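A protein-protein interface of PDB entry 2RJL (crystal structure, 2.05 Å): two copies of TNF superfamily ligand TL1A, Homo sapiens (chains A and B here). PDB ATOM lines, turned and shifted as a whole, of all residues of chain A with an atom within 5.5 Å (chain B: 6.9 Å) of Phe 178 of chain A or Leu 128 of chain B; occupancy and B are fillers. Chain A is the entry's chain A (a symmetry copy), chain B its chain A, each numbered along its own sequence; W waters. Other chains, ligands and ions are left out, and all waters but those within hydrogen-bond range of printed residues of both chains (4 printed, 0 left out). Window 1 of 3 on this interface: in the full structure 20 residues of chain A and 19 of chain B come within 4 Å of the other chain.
O of Met 129 of chain B lies within hydrogen-bond range of NE2 of Gln 85 of chain A (3.0 Å).
OH of Tyr 83 of chain A sits at hydrogen-bond distance from N of Met 150 of chain B.
The backbone NH of Met 129 of chain B sits at hydrogen-bond distance from the backbone carbonyl oxygen of Asp 175 of chain A, at 2.8 Å.
The side-chain amide nitrogen of Gln 126 of chain B is in hydrogen-bond range of the side-chain carboxylate of Asp 175 of chain A.
The backbone carbonyl oxygen (O) of Gly 148 of chain B lies within hydrogen-bond range of the side-chain hydroxyl (OH) of Tyr 146 of chain A (2.7 Å).
A ring nitrogen (ND1) of His 31 of chain A lies within hydrogen-bond range of the side-chain hydroxyl (OH) of Tyr 83 of chain A (2.8 Å).
O of Leu 147 of chain B lies within hydrogen-bond range of N of Ser 84 of chain B, 2.9 Å away.
The backbone carbonyl oxygen (O) of Tyr 83 of chain A lies within hydrogen-bond range of the backbone NH (N) of Gly 180 of chain A.
Among the printed residues, pairs that only touch across the chains: Asp 175 of chain A with Leu 127 of chain B (3.4 Å), Phe 178 of chain A with Leu 128 of chain B (3.4 Å), Gln 85 of chain A with Leu 147 of chain B (3.5 Å), His 31 of chain A with Met 150 of chain B (3.5 Å), Tyr 83 of chain A with Ala 149 of chain B (3.5 Å), Asp 175 of chain A with Leu 128 of chain B (3.6 Å), Tyr 146 of chain A with Tyr 146 of chain B (3.6 Å), His 31 of chain A with Ala 149 of chain B (3.6 Å), His 31 of chain A with Phe 151 of chain B (3.7 Å), Tyr 83 of chain A with Gly 148 of chain B (3.9 Å), Phe 178 of chain A with Gly 148 of chain B (3.9 Å), Lys 176 of chain A with Met 129 of chain B (3.9 Å) and Gln 85 of chain A with Tyr 146 of chain B (3.997 Å).
Of chain B, only Leu 128 and Gly 148 come within 4 Å of Phe 178 of chain A.
Of chain A, only Asp 175 (3.6 Å) and Phe 178 (3.4 Å) come within 4 Å of Leu 128 of chain B.
Of the printed residues of chain A, Met 150 of chain B touches His 31 and Tyr 83.
Of the printed residues of chain B, Asp 175 of chain A touches Gln 126 (2.8 Å), Leu 127 (3.4 Å), Leu 128 (3.6 Å) and Met 129 (2.8 Å).
Printed residues of chain B within 4 Å of Gln 85 of chain A: Met 129, Tyr 146 and Leu 147.
Gly 130 of chain B touches none of the printed residues of chain A.
Tyr 83 of chain B touches none of the printed residues of chain A.
The nearest residue of chain B that does not touch Phe 178 of chain A is Ala 149 of chain B (4.05 Å).
The nearest printed residue of chain B that does not touch Tyr 83 of chain A is Phe 151 of chain B (5.5 Å).
Hydrophobic or aromatic side chains of chain B that line the printed part of chain A: Leu 128, Met 129, Tyr 146, Leu 147, Ala 149, Met 150 and Phe 151.
Of the 17 printed residues of chain A, 7 touch a printed residue of chain B.
Hydrophobic or aromatic side chains of chain A within 4 Å of the printed part of chain B: His 31, Tyr 83, Tyr 146 and Phe 178.
Among the printed residues, 18 pairs touch across the chains.
Tyr 146 of chain A touches its own counterpart, Tyr 146 of chain B.
3 positions are printed for both chains.
Of the 18 pairs that touch across the chains among the printed residues, 1 has its exchanged pair printed and touching as well.
Water W1 bridges the side-chain carboxylate (OD1) of Asp 175 of chain A (2.7 Å) and the side-chain sulfur (SD) of Met 129 of chain B (3.1 Å).
Water W4 lies within hydrogen-bond range of a ring nitrogen (NE2) of His 31 of chain A, the backbone carbonyl oxygen (O) of Leu 127 of chain B and the backbone carbonyl oxygen (O) of Glu 174 of chain A.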
ATOM      1  N   HIS A  31      -2.415  23.091 -21.345  1.00  0.00           N
ATOM      2  CA  HIS A  31      -3.218  23.526 -20.220  1.00  0.00           C
ATOM      3  C   HIS A  31      -4.663  23.266 -20.562  1.00  0.00           C
ATOM      4  O   HIS A  31      -5.170  23.815 -21.537  1.00  0.00           O
ATOM      5  CB  HIS A  31      -3.050  25.033 -19.998  1.00  0.00           C
ATOM      6  CG  HIS A  31      -3.850  25.568 -18.853  1.00  0.00           C
ATOM      7  ND1 HIS A  31      -3.586  25.226 -17.543  1.00  0.00           N
ATOM      8  CD2 HIS A  31      -4.906  26.418 -18.816  1.00  0.00           C
ATOM      9  CE1 HIS A  31      -4.427  25.866 -16.744  1.00  0.00           C
ATOM     10  NE2 HIS A  31      -5.243  26.589 -17.492  1.00  0.00           N
ATOM     11  N   LEU A  32      -5.338  22.435 -19.776  1.00  0.00           N
ATOM     12  CA  LEU A  32      -6.736  22.069 -20.117  1.00  0.00           C
ATOM     13  C   LEU A  32      -7.677  22.637 -19.065  1.00  0.00           C
ATOM     14  O   LEU A  32      -7.284  22.789 -17.912  1.00  0.00           O
ATOM     15  CB  LEU A  32      -6.887  20.540 -20.202  1.00  0.00           C
ATOM     16  CG  LEU A  32      -5.821  19.797 -21.010  1.00  0.00           C
ATOM     17  CD1 LEU A  32      -6.031  18.270 -20.867  1.00  0.00           C
ATOM     18  CD2 LEU A  32      -5.924  20.229 -22.463  1.00  0.00           C
ATOM     19  N   THR A  33      -8.890  23.001 -19.473  1.00  0.00           N
ATOM     20  CA  THR A  33      -9.818  23.683 -18.579  1.00  0.00           C
ATOM     21  C   THR A  33     -11.155  22.950 -18.490  1.00  0.00           C
ATOM     22  O   THR A  33     -11.525  22.176 -19.381  1.00  0.00           O
ATOM     23  CB  THR A  33     -10.037  25.174 -18.978  1.00  0.00           C
ATOM     24  OG1 THR A  33     -10.648  25.237 -20.272  1.00  0.00           O
ATOM     25  CG2 THR A  33      -8.708  25.922 -19.030  1.00  0.00           C
ATOM     26  N   VAL A  34     -11.870  23.169 -17.393  1.00  0.00           N
ATOM     27  CA  VAL A  34     -13.035  22.351 -17.092  1.00  0.00           C
ATOM     28  C   VAL A  34     -14.169  22.640 -18.083  1.00  0.00           C
ATOM     29  O   VAL A  34     -14.255  23.737 -18.643  1.00  0.00           O
ATOM     30  CB  VAL A  34     -13.510  22.610 -15.665  1.00  0.00           C
ATOM     31  CG1 VAL A  34     -14.124  24.000 -15.566  1.00  0.00           C
ATOM     32  CG2 VAL A  34     -14.463  21.505 -15.175  1.00  0.00           C
ATOM     33  N   TRP A  52     -12.207  17.462 -20.629  1.00  0.00           N
ATOM     34  CA  TRP A  52     -11.669  18.829 -20.564  1.00  0.00           C
ATOM     35  C   TRP A  52     -11.873  19.583 -21.867  1.00  0.00           C
ATOM     36  O   TRP A  52     -11.973  18.968 -22.920  1.00  0.00           O
ATOM     37  CB  TRP A  52     -10.168  18.757 -20.309  1.00  0.00           C
ATOM     38  CG  TRP A  52      -9.838  18.027 -19.040  1.00  0.00           C
ATOM     39  CD1 TRP A  52      -9.503  16.716 -18.897  1.00  0.00           C
ATOM     40  CD2 TRP A  52      -9.835  18.593 -17.729  1.00  0.00           C
ATOM     41  NE1 TRP A  52      -9.297  16.419 -17.548  1.00  0.00           N
ATOM     42  CE2 TRP A  52      -9.501  17.564 -16.820  1.00  0.00           C
ATOM     43  CE3 TRP A  52     -10.077  19.873 -17.233  1.00  0.00           C
ATOM     44  CZ2 TRP A  52      -9.397  17.792 -15.441  1.00  0.00           C
ATOM     45  CZ3 TRP A  52      -9.984  20.090 -15.859  1.00  0.00           C
ATOM     46  CH2 TRP A  52      -9.634  19.064 -14.988  1.00  0.00           C
ATOM     47  N   TYR A  83       0.044  19.109 -13.254  1.00  0.00           N
ATOM     48  CA  TYR A  83      -0.723  19.845 -12.249  1.00  0.00           C
ATOM     49  C   TYR A  83      -2.215  19.817 -12.509  1.00  0.00           C
ATOM     50  O   TYR A  83      -2.649  19.663 -13.654  1.00  0.00           O
ATOM     51  CB  TYR A  83      -0.258  21.307 -12.125  1.00  0.00           C
ATOM     52  CG  TYR A  83      -0.468  22.146 -13.387  1.00  0.00           C
ATOM     53  CD1 TYR A  83      -1.697  22.756 -13.656  1.00  0.00           C
ATOM     54  CD2 TYR A  83       0.558  22.324 -14.303  1.00  0.00           C
ATOM     55  CE1 TYR A  83      -1.894  23.522 -14.806  1.00  0.00           C
ATOM     56  CE2 TYR A  83       0.366  23.089 -15.464  1.00  0.00           C
ATOM     57  CZ  TYR A  83      -0.856  23.687 -15.695  1.00  0.00           C
ATOM     58  OH  TYR A  83      -1.040  24.466 -16.807  1.00  0.00           O
ATOM     59  N   SER A  84      -2.999  19.987 -11.442  1.00  0.00           N
ATOM     60  CA  SER A  84      -4.448  20.142 -11.585  1.00  0.00           C
ATOM     61  C   SER A  84      -4.989  20.861 -10.360  1.00  0.00           C
ATOM     62  O   SER A  84      -4.493  20.673  -9.239  1.00  0.00           O
ATOM     63  CB  SER A  84      -5.130  18.764 -11.726  1.00  0.00           C
ATOM     64  OG  SER A  84      -6.532  18.886 -11.953  1.00  0.00           O
ATOM     65  N   GLN A  85      -6.000  21.694 -10.583  1.00  0.00           N
ATOM     66  CA  GLN A  85      -6.916  22.073  -9.522  1.00  0.00           C
ATOM     67  C   GLN A  85      -8.317  21.653  -9.884  1.00  0.00           C
ATOM     68  O   GLN A  85      -8.751  21.826 -11.021  1.00  0.00           O
ATOM     69  CB  GLN A  85      -6.894  23.578  -9.296  1.00  0.00           C
ATOM     70  CG  GLN A  85      -7.881  24.022  -8.235  1.00  0.00           C
ATOM     71  CD  GLN A  85      -7.710  25.456  -7.895  1.00  0.00           C
ATOM     72  OE1 GLN A  85      -6.929  25.787  -7.002  1.00  0.00           O
ATOM     73  NE2 GLN A  85      -8.431  26.346  -8.615  1.00  0.00           N
ATOM     74  N   VAL A  86      -9.009  21.079  -8.913  1.00  0.00           N
ATOM     75  CA  VAL A  86     -10.437  20.872  -9.008  1.00  0.00           C
ATOM     76  C   VAL A  86     -11.085  21.637  -7.871  1.00  0.00           C
ATOM     77  O   VAL A  86     -10.762  21.435  -6.698  1.00  0.00           O
ATOM     78  CB  VAL A  86     -10.782  19.383  -8.916  1.00  0.00           C
ATOM     79  CG1 VAL A  86     -12.308  19.172  -9.000  1.00  0.00           C
ATOM     80  CG2 VAL A  86     -10.086  18.641 -10.042  1.00  0.00           C
ATOM     81  N   TYR A 146      -5.595  21.647  -5.067  1.00  0.00           N
ATOM     82  CA  TYR A 146      -4.536  21.850  -6.059  1.00  0.00           C
ATOM     83  C   TYR A 146      -3.386  20.862  -5.801  1.00  0.00           C
ATOM     84  O   TYR A 146      -2.960  20.680  -4.661  1.00  0.00           O
ATOM     85  CB  TYR A 146      -3.997  23.294  -6.001  1.00  0.00           C
ATOM     86  CG  TYR A 146      -2.908  23.527  -7.022  1.00  0.00           C
ATOM     87  CD1 TYR A 146      -3.217  24.053  -8.273  1.00  0.00           C
ATOM     88  CD2 TYR A 146      -1.590  23.124  -6.772  1.00  0.00           C
ATOM     89  CE1 TYR A 146      -2.244  24.201  -9.233  1.00  0.00           C
ATOM     90  CE2 TYR A 146      -0.603  23.284  -7.718  1.00  0.00           C
ATOM     91  CZ  TYR A 146      -0.940  23.836  -8.945  1.00  0.00           C
ATOM     92  OH  TYR A 146       0.010  24.004  -9.888  1.00  0.00           O
ATOM     93  N   GLU A 174     -13.310  28.482 -16.469  1.00  0.00           N
ATOM     94  CA  GLU A 174     -12.039  27.861 -16.882  1.00  0.00           C
ATOM     95  C   GLU A 174     -10.896  28.116 -15.884  1.00  0.00           C
ATOM     96  O   GLU A 174      -9.882  27.418 -15.904  1.00  0.00           O
ATOM     97  CB  GLU A 174     -11.631  28.374 -18.274  1.00  0.00           C
ATOM     98  CG  GLU A 174     -11.427  29.888 -18.306  1.00  0.00           C
ATOM     99  CD  GLU A 174     -10.952  30.431 -19.644  1.00  0.00           C
ATOM    100  OE1 GLU A 174     -10.528  29.650 -20.544  1.00  0.00           O
ATOM    101  OE2 GLU A 174     -10.984  31.667 -19.778  1.00  0.00           O
ATOM    102  N   ASP A 175     -11.054  29.120 -15.024  1.00  0.00           N
ATOM    103  CA  ASP A 175     -10.000  29.475 -14.074  1.00  0.00           C
ATOM    104  C   ASP A 175     -10.091  28.744 -12.738  1.00  0.00           C
ATOM    105  O   ASP A 175      -9.187  28.848 -11.895  1.00  0.00           O
ATOM    106  CB  ASP A 175      -9.894  31.000 -13.883  1.00  0.00           C
ATOM    107  CG  ASP A 175     -11.182  31.630 -13.350  1.00  0.00           C
ATOM    108  OD1 ASP A 175     -12.259  31.046 -13.502  1.00  0.00           O
ATOM    109  OD2 ASP A 175     -11.118  32.722 -12.768  1.00  0.00           O
ATOM    110  N   LYS A 176     -11.161  27.978 -12.541  1.00  0.00           N
ATOM    111  CA  LYS A 176     -11.350  27.308 -11.252  1.00  0.00           C
ATOM    112  C   LYS A 176     -10.992  25.827 -11.230  1.00  0.00           C
ATOM    113  O   LYS A 176     -10.674  25.278 -10.177  1.00  0.00           O
ATOM    114  CB  LYS A 176     -12.792  27.445 -10.788  1.00  0.00           C
ATOM    115  CG  LYS A 176     -13.133  28.847 -10.248  1.00  0.00           C
ATOM    116  CD  LYS A 176     -14.439  28.779  -9.464  1.00  0.00           C
ATOM    117  CE  LYS A 176     -15.596  29.355 -10.235  1.00  0.00           C
ATOM    118  NZ  LYS A 176     -16.868  29.278  -9.428  1.00  0.00           N
ATOM    119  N   THR A 177     -11.091  25.163 -12.375  1.00  0.00           N
ATOM    120  CA  THR A 177     -10.802  23.721 -12.441  1.00  0.00           C
ATOM    121  C   THR A 177     -10.035  23.512 -13.751  1.00  0.00           C
ATOM    122  O   THR A 177     -10.488  23.939 -14.808  1.00  0.00           O
ATOM    123  CB  THR A 177     -12.089  22.876 -12.412  1.00  0.00           C
ATOM    124  OG1 THR A 177     -12.759  23.076 -11.169  1.00  0.00           O
ATOM    125  CG2 THR A 177     -11.794  21.363 -12.553  1.00  0.00           C
ATOM    126  N   PHE A 178      -8.857  22.902 -13.664  1.00  0.00           N
ATOM    127  CA  PHE A 178      -7.912  22.855 -14.792  1.00  0.00           C
ATOM    128  C   PHE A 178      -6.898  21.754 -14.564  1.00  0.00           C
ATOM    129  O   PHE A 178      -6.811  21.191 -13.462  1.00  0.00           O
ATOM    130  CB  PHE A 178      -7.190  24.205 -15.007  1.00  0.00           C
ATOM    131  CG  PHE A 178      -6.585  24.786 -13.755  1.00  0.00           C
ATOM    132  CD1 PHE A 178      -5.351  24.355 -13.298  1.00  0.00           C
ATOM    133  CD2 PHE A 178      -7.253  25.770 -13.052  1.00  0.00           C
ATOM    134  CE1 PHE A 178      -4.795  24.889 -12.144  1.00  0.00           C
ATOM    135  CE2 PHE A 178      -6.712  26.315 -11.899  1.00  0.00           C
ATOM    136  CZ  PHE A 178      -5.480  25.872 -11.442  1.00  0.00           C
ATOM    137  N   PHE A 179      -6.142  21.436 -15.607  1.00  0.00           N
ATOM    138  CA  PHE A 179      -5.274  20.249 -15.621  1.00  0.00           C
ATOM    139  C   PHE A 179      -4.218  20.548 -16.686  1.00  0.00           C
ATOM    140  O   PHE A 179      -4.563  20.875 -17.816  1.00  0.00           O
ATOM    141  CB  PHE A 179      -6.114  19.020 -16.007  1.00  0.00           C
ATOM    142  CG  PHE A 179      -5.312  17.745 -16.324  1.00  0.00           C
ATOM    143  CD1 PHE A 179      -4.163  17.401 -15.609  1.00  0.00           C
ATOM    144  CD2 PHE A 179      -5.771  16.862 -17.302  1.00  0.00           C
ATOM    145  CE1 PHE A 179      -3.464  16.210 -15.889  1.00  0.00           C
ATOM    146  CE2 PHE A 179      -5.071  15.669 -17.603  1.00  0.00           C
ATOM    147  CZ  PHE A 179      -3.914  15.353 -16.901  1.00  0.00           C
ATOM    148  N   GLY A 180      -2.938  20.477 -16.330  1.00  0.00           N
ATOM    149  CA  GLY A 180      -1.886  20.808 -17.306  1.00  0.00           C
ATOM    150  C   GLY A 180      -0.623  19.976 -17.136  1.00  0.00           C
ATOM    151  O   GLY A 180      -0.463  19.278 -16.136  1.00  0.00           O
ATOM    152  N   ILE B  82       2.899  30.381 -13.870  1.00  0.00           N
ATOM    153  CA  ILE B  82       2.535  31.465 -12.952  1.00  0.00           C
ATOM    154  C   ILE B  82       2.126  30.802 -11.638  1.00  0.00           C
ATOM    155  O   ILE B  82       1.712  29.645 -11.644  1.00  0.00           O
ATOM    156  CB  ILE B  82       1.351  32.277 -13.533  1.00  0.00           C
ATOM    157  CG1 ILE B  82       1.577  32.542 -15.035  1.00  0.00           C
ATOM    158  CG2 ILE B  82       1.126  33.574 -12.758  1.00  0.00           C
ATOM    159  CD1 ILE B  82       0.758  33.687 -15.583  1.00  0.00           C
ATOM    160  N   TYR B  83       2.262  31.502 -10.516  1.00  0.00           N
ATOM    161  CA  TYR B  83       1.830  30.938  -9.238  1.00  0.00           C
ATOM    162  C   TYR B  83       1.643  31.988  -8.163  1.00  0.00           C
ATOM    163  O   TYR B  83       2.266  33.052  -8.211  1.00  0.00           O
ATOM    164  CB  TYR B  83       2.802  29.858  -8.727  1.00  0.00           C
ATOM    165  CG  TYR B  83       4.208  30.372  -8.409  1.00  0.00           C
ATOM    166  CD1 TYR B  83       4.504  30.957  -7.174  1.00  0.00           C
ATOM    167  CD2 TYR B  83       5.230  30.272  -9.341  1.00  0.00           C
ATOM    168  CE1 TYR B  83       5.784  31.428  -6.880  1.00  0.00           C
ATOM    169  CE2 TYR B  83       6.518  30.748  -9.054  1.00  0.00           C
ATOM    170  CZ  TYR B  83       6.781  31.311  -7.821  1.00  0.00           C
ATOM    171  OH  TYR B  83       8.046  31.743  -7.519  1.00  0.00           O
ATOM    172  N   SER B  84       0.795  31.676  -7.180  1.00  0.00           N
ATOM    173  CA  SER B  84       0.653  32.536  -6.003  1.00  0.00           C
ATOM    174  C   SER B  84       0.106  31.706  -4.852  1.00  0.00           C
ATOM    175  O   SER B  84      -0.707  30.791  -5.055  1.00  0.00           O
ATOM    176  CB  SER B  84      -0.303  33.710  -6.301  1.00  0.00           C
ATOM    177  OG  SER B  84      -0.396  34.612  -5.202  1.00  0.00           O
ATOM    178  N   VAL B 112      -8.613  34.212  -4.060  1.00  0.00           N
ATOM    179  CA  VAL B 112      -7.480  34.756  -4.805  1.00  0.00           C
ATOM    180  C   VAL B 112      -7.709  34.558  -6.308  1.00  0.00           C
ATOM    181  O   VAL B 112      -8.104  33.483  -6.741  1.00  0.00           O
ATOM    182  CB  VAL B 112      -6.168  33.953  -4.523  1.00  0.00           C
ATOM    183  CG1 VAL B 112      -4.948  34.705  -5.110  1.00  0.00           C
ATOM    184  CG2 VAL B 112      -5.975  33.713  -3.075  1.00  0.00           C
ATOM    185  N   VAL B 113      -7.425  35.586  -7.100  1.00  0.00           N
ATOM    186  CA  VAL B 113      -7.581  35.519  -8.541  1.00  0.00           C
ATOM    187  C   VAL B 113      -6.284  36.065  -9.101  1.00  0.00           C
ATOM    188  O   VAL B 113      -5.781  37.094  -8.640  1.00  0.00           O
ATOM    189  CB  VAL B 113      -8.715  36.431  -9.035  1.00  0.00           C
ATOM    190  CG1 VAL B 113      -8.918  36.219 -10.530  1.00  0.00           C
ATOM    191  CG2 VAL B 113      -9.986  36.138  -8.289  1.00  0.00           C
ATOM    192  N   ILE B 114      -5.701  35.355 -10.052  1.00  0.00           N
ATOM    193  CA  ILE B 114      -4.584  35.918 -10.796  1.00  0.00           C
ATOM    194  C   ILE B 114      -5.104  36.343 -12.163  1.00  0.00           C
ATOM    195  O   ILE B 114      -5.774  35.570 -12.847  1.00  0.00           O
ATOM    196  CB  ILE B 114      -3.430  34.895 -10.958  1.00  0.00           C
ATOM    197  CG1 ILE B 114      -2.865  34.490  -9.587  1.00  0.00           C
ATOM    198  CG2 ILE B 114      -2.291  35.498 -11.805  1.00  0.00           C
ATOM    199  CD1 ILE B 114      -1.781  33.412  -9.698  1.00  0.00           C
ATOM    200  N   THR B 115      -4.808  37.581 -12.532  1.00  0.00           N
ATOM    201  CA  THR B 115      -5.466  38.245 -13.666  1.00  0.00           C
ATOM    202  C   THR B 115      -4.405  38.748 -14.654  1.00  0.00           C
ATOM    203  O   THR B 115      -3.323  39.179 -14.241  1.00  0.00           O
ATOM    204  CB  THR B 115      -6.264  39.461 -13.137  1.00  0.00           C
ATOM    205  OG1 THR B 115      -7.352  38.985 -12.329  1.00  0.00           O
ATOM    206  CG2 THR B 115      -6.806  40.296 -14.254  1.00  0.00           C
ATOM    207  N   THR B 125      -8.383  39.366 -18.080  1.00  0.00           N
ATOM    208  CA  THR B 125      -8.721  37.946 -18.147  1.00  0.00           C
ATOM    209  C   THR B 125      -8.296  37.235 -16.871  1.00  0.00           C
ATOM    210  O   THR B 125      -7.127  37.315 -16.473  1.00  0.00           O
ATOM    211  CB  THR B 125      -8.036  37.298 -19.369  1.00  0.00           C
ATOM    212  OG1 THR B 125      -8.383  38.032 -20.544  1.00  0.00           O
ATOM    213  CG2 THR B 125      -8.461  35.851 -19.545  1.00  0.00           C
ATOM    214  N   GLN B 126      -9.244  36.557 -16.225  1.00  0.00           N
ATOM    215  CA  GLN B 126      -8.961  35.747 -15.049  1.00  0.00           C
ATOM    216  C   GLN B 126      -8.304  34.452 -15.524  1.00  0.00           C
ATOM    217  O   GLN B 126      -8.906  33.681 -16.273  1.00  0.00           O
ATOM    218  CB  GLN B 126     -10.255  35.442 -14.269  1.00  0.00           C
ATOM    219  CG  GLN B 126     -10.820  36.669 -13.572  1.00  0.00           C
ATOM    220  CD  GLN B 126     -12.134  36.433 -12.845  1.00  0.00           C
ATOM    221  OE1 GLN B 126     -12.875  37.377 -12.594  1.00  0.00           O
ATOM    222  NE2 GLN B 126     -12.428  35.181 -12.501  1.00  0.00           N
ATOM    223  N   LEU B 127      -7.069  34.229 -15.081  1.00  0.00           N
ATOM    224  CA  LEU B 127      -6.307  33.050 -15.460  1.00  0.00           C
ATOM    225  C   LEU B 127      -6.537  31.903 -14.463  1.00  0.00           C
ATOM    226  O   LEU B 127      -6.665  30.741 -14.844  1.00  0.00           O
ATOM    227  CB  LEU B 127      -4.812  33.411 -15.482  1.00  0.00           C
ATOM    228  CG  LEU B 127      -4.391  34.553 -16.411  1.00  0.00           C
ATOM    229  CD1 LEU B 127      -2.874  34.655 -16.374  1.00  0.00           C
ATOM    230  CD2 LEU B 127      -4.863  34.288 -17.868  1.00  0.00           C
ATOM    231  N   LEU B 128      -6.588  32.252 -13.184  1.00  0.00           N
ATOM    232  CA  LEU B 128      -6.555  31.273 -12.087  1.00  0.00           C
ATOM    233  C   LEU B 128      -7.398  31.809 -10.954  1.00  0.00           C
ATOM    234  O   LEU B 128      -7.247  32.961 -10.583  1.00  0.00           O
ATOM    235  CB  LEU B 128      -5.128  31.137 -11.549  1.00  0.00           C
ATOM    236  CG  LEU B 128      -4.150  30.405 -12.457  1.00  0.00           C
ATOM    237  CD1 LEU B 128      -2.719  30.519 -11.956  1.00  0.00           C
ATOM    238  CD2 LEU B 128      -4.591  28.946 -12.535  1.00  0.00           C
ATOM    239  N   MET B 129      -8.255  30.977 -10.375  1.00  0.00           N
ATOM    240  CA  MET B 129      -9.025  31.418  -9.225  1.00  0.00           C
ATOM    241  C   MET B 129      -9.073  30.339  -8.150  1.00  0.00           C
ATOM    242  O   MET B 129      -9.405  29.175  -8.433  1.00  0.00           O
ATOM    243  CB  MET B 129     -10.448  31.838  -9.630  1.00  0.00           C
ATOM    244  CG  MET B 129     -11.375  32.007  -8.409  1.00  0.00           C
ATOM    245  SD  MET B 129     -13.025  32.653  -8.798  1.00  0.00           S
ATOM    246  CE  MET B 129     -12.698  34.328  -9.301  1.00  0.00           C
ATOM    247  N   GLY B 130      -8.743  30.727  -6.919  1.00  0.00           N
ATOM    248  CA  GLY B 130      -8.893  29.821  -5.777  1.00  0.00           C
ATOM    249  C   GLY B 130      -9.851  30.466  -4.814  1.00  0.00           C
ATOM    250  O   GLY B 130      -9.604  31.560  -4.306  1.00  0.00           O
ATOM    251  N   TYR B 146      -3.350  28.272  -2.558  1.00  0.00           N
ATOM    252  CA  TYR B 146      -2.249  28.189  -3.521  1.00  0.00           C
ATOM    253  C   TYR B 146      -2.801  27.846  -4.915  1.00  0.00           C
ATOM    254  O   TYR B 146      -3.640  26.957  -5.055  1.00  0.00           O
ATOM    255  CB  TYR B 146      -1.224  27.118  -3.095  1.00  0.00           C
ATOM    256  CG  TYR B 146      -0.075  27.022  -4.071  1.00  0.00           C
ATOM    257  CD1 TYR B 146       1.096  27.742  -3.854  1.00  0.00           C
ATOM    258  CD2 TYR B 146      -0.202  26.294  -5.262  1.00  0.00           C
ATOM    259  CE1 TYR B 146       2.118  27.717  -4.773  1.00  0.00           C
ATOM    260  CE2 TYR B 146       0.821  26.246  -6.181  1.00  0.00           C
ATOM    261  CZ  TYR B 146       1.985  26.954  -5.921  1.00  0.00           C
ATOM    262  OH  TYR B 146       3.002  26.922  -6.806  1.00  0.00           O
ATOM    263  N   LEU B 147      -2.270  28.511  -5.938  1.00  0.00           N
ATOM    264  CA  LEU B 147      -2.678  28.323  -7.337  1.00  0.00           C
ATOM    265  C   LEU B 147      -1.416  28.416  -8.184  1.00  0.00           C
ATOM    266  O   LEU B 147      -0.580  29.264  -7.918  1.00  0.00           O
ATOM    267  CB  LEU B 147      -3.533  29.537  -7.779  1.00  0.00           C
ATOM    268  CG  LEU B 147      -4.936  29.776  -7.264  1.00  0.00           C
ATOM    269  CD1 LEU B 147      -5.314  31.272  -7.327  1.00  0.00           C
ATOM    270  CD2 LEU B 147      -5.893  28.937  -8.115  1.00  0.00           C
ATOM    271  N   GLY B 148      -1.309  27.602  -9.234  1.00  0.00           N
ATOM    272  CA  GLY B 148      -0.222  27.751 -10.229  1.00  0.00           C
ATOM    273  C   GLY B 148      -0.551  27.006 -11.512  1.00  0.00           C
ATOM    274  O   GLY B 148      -1.102  25.896 -11.482  1.00  0.00           O
ATOM    275  N   ALA B 149      -0.227  27.590 -12.650  1.00  0.00           N
ATOM    276  CA  ALA B 149      -0.525  26.922 -13.918  1.00  0.00           C
ATOM    277  C   ALA B 149       0.272  27.612 -15.017  1.00  0.00           C
ATOM    278  O   ALA B 149       0.880  28.663 -14.786  1.00  0.00           O
ATOM    279  CB  ALA B 149      -2.047  26.996 -14.235  1.00  0.00           C
ATOM    280  N   MET B 150       0.251  27.002 -16.193  1.00  0.00           N
ATOM    281  CA  MET B 150       0.959  27.491 -17.378  1.00  0.00           C
ATOM    282  C   MET B 150       0.013  28.224 -18.342  1.00  0.00           C
ATOM    283  O   MET B 150      -1.094  27.747 -18.625  1.00  0.00           O
ATOM    284  CB  MET B 150       1.621  26.312 -18.088  1.00  0.00           C
ATOM    285  CG  MET B 150       2.081  26.597 -19.559  1.00  0.00           C
ATOM    286  SD  MET B 150       2.746  25.081 -20.236  1.00  0.00           S
ATOM    287  CE  MET B 150       1.346  23.993 -20.213  1.00  0.00           C
ATOM    288  N   PHE B 151       0.447  29.393 -18.827  1.00  0.00           N
ATOM    289  CA  PHE B 151      -0.364  30.229 -19.733  1.00  0.00           C
ATOM    290  C   PHE B 151       0.523  30.783 -20.833  1.00  0.00           C
ATOM    291  O   PHE B 151       1.702  31.054 -20.605  1.00  0.00           O
ATOM    292  CB  PHE B 151      -1.029  31.397 -18.966  1.00  0.00           C
ATOM    293  CG  PHE B 151      -1.998  30.930 -17.921  1.00  0.00           C
ATOM    294  CD1 PHE B 151      -3.299  30.611 -18.262  1.00  0.00           C
ATOM    295  CD2 PHE B 151      -1.582  30.726 -16.619  1.00  0.00           C
ATOM    296  CE1 PHE B 151      -4.186  30.116 -17.313  1.00  0.00           C
ATOM    297  CE2 PHE B 151      -2.469  30.259 -15.672  1.00  0.00           C
ATOM    298  CZ  PHE B 151      -3.751  29.937 -16.022  1.00  0.00           C
HETATM  299  O   HOH W   1     -13.978  31.971 -11.618  1.00  0.00           O
HETATM  300  O   HOH W   2      -6.251  26.570  -4.663  1.00  0.00           O
HETATM  301  O   HOH W   3     -11.171  33.380 -17.622  1.00  0.00           O
HETATM  302  O   HOH W   4      -7.165  28.356 -16.352  1.00  0.00           O
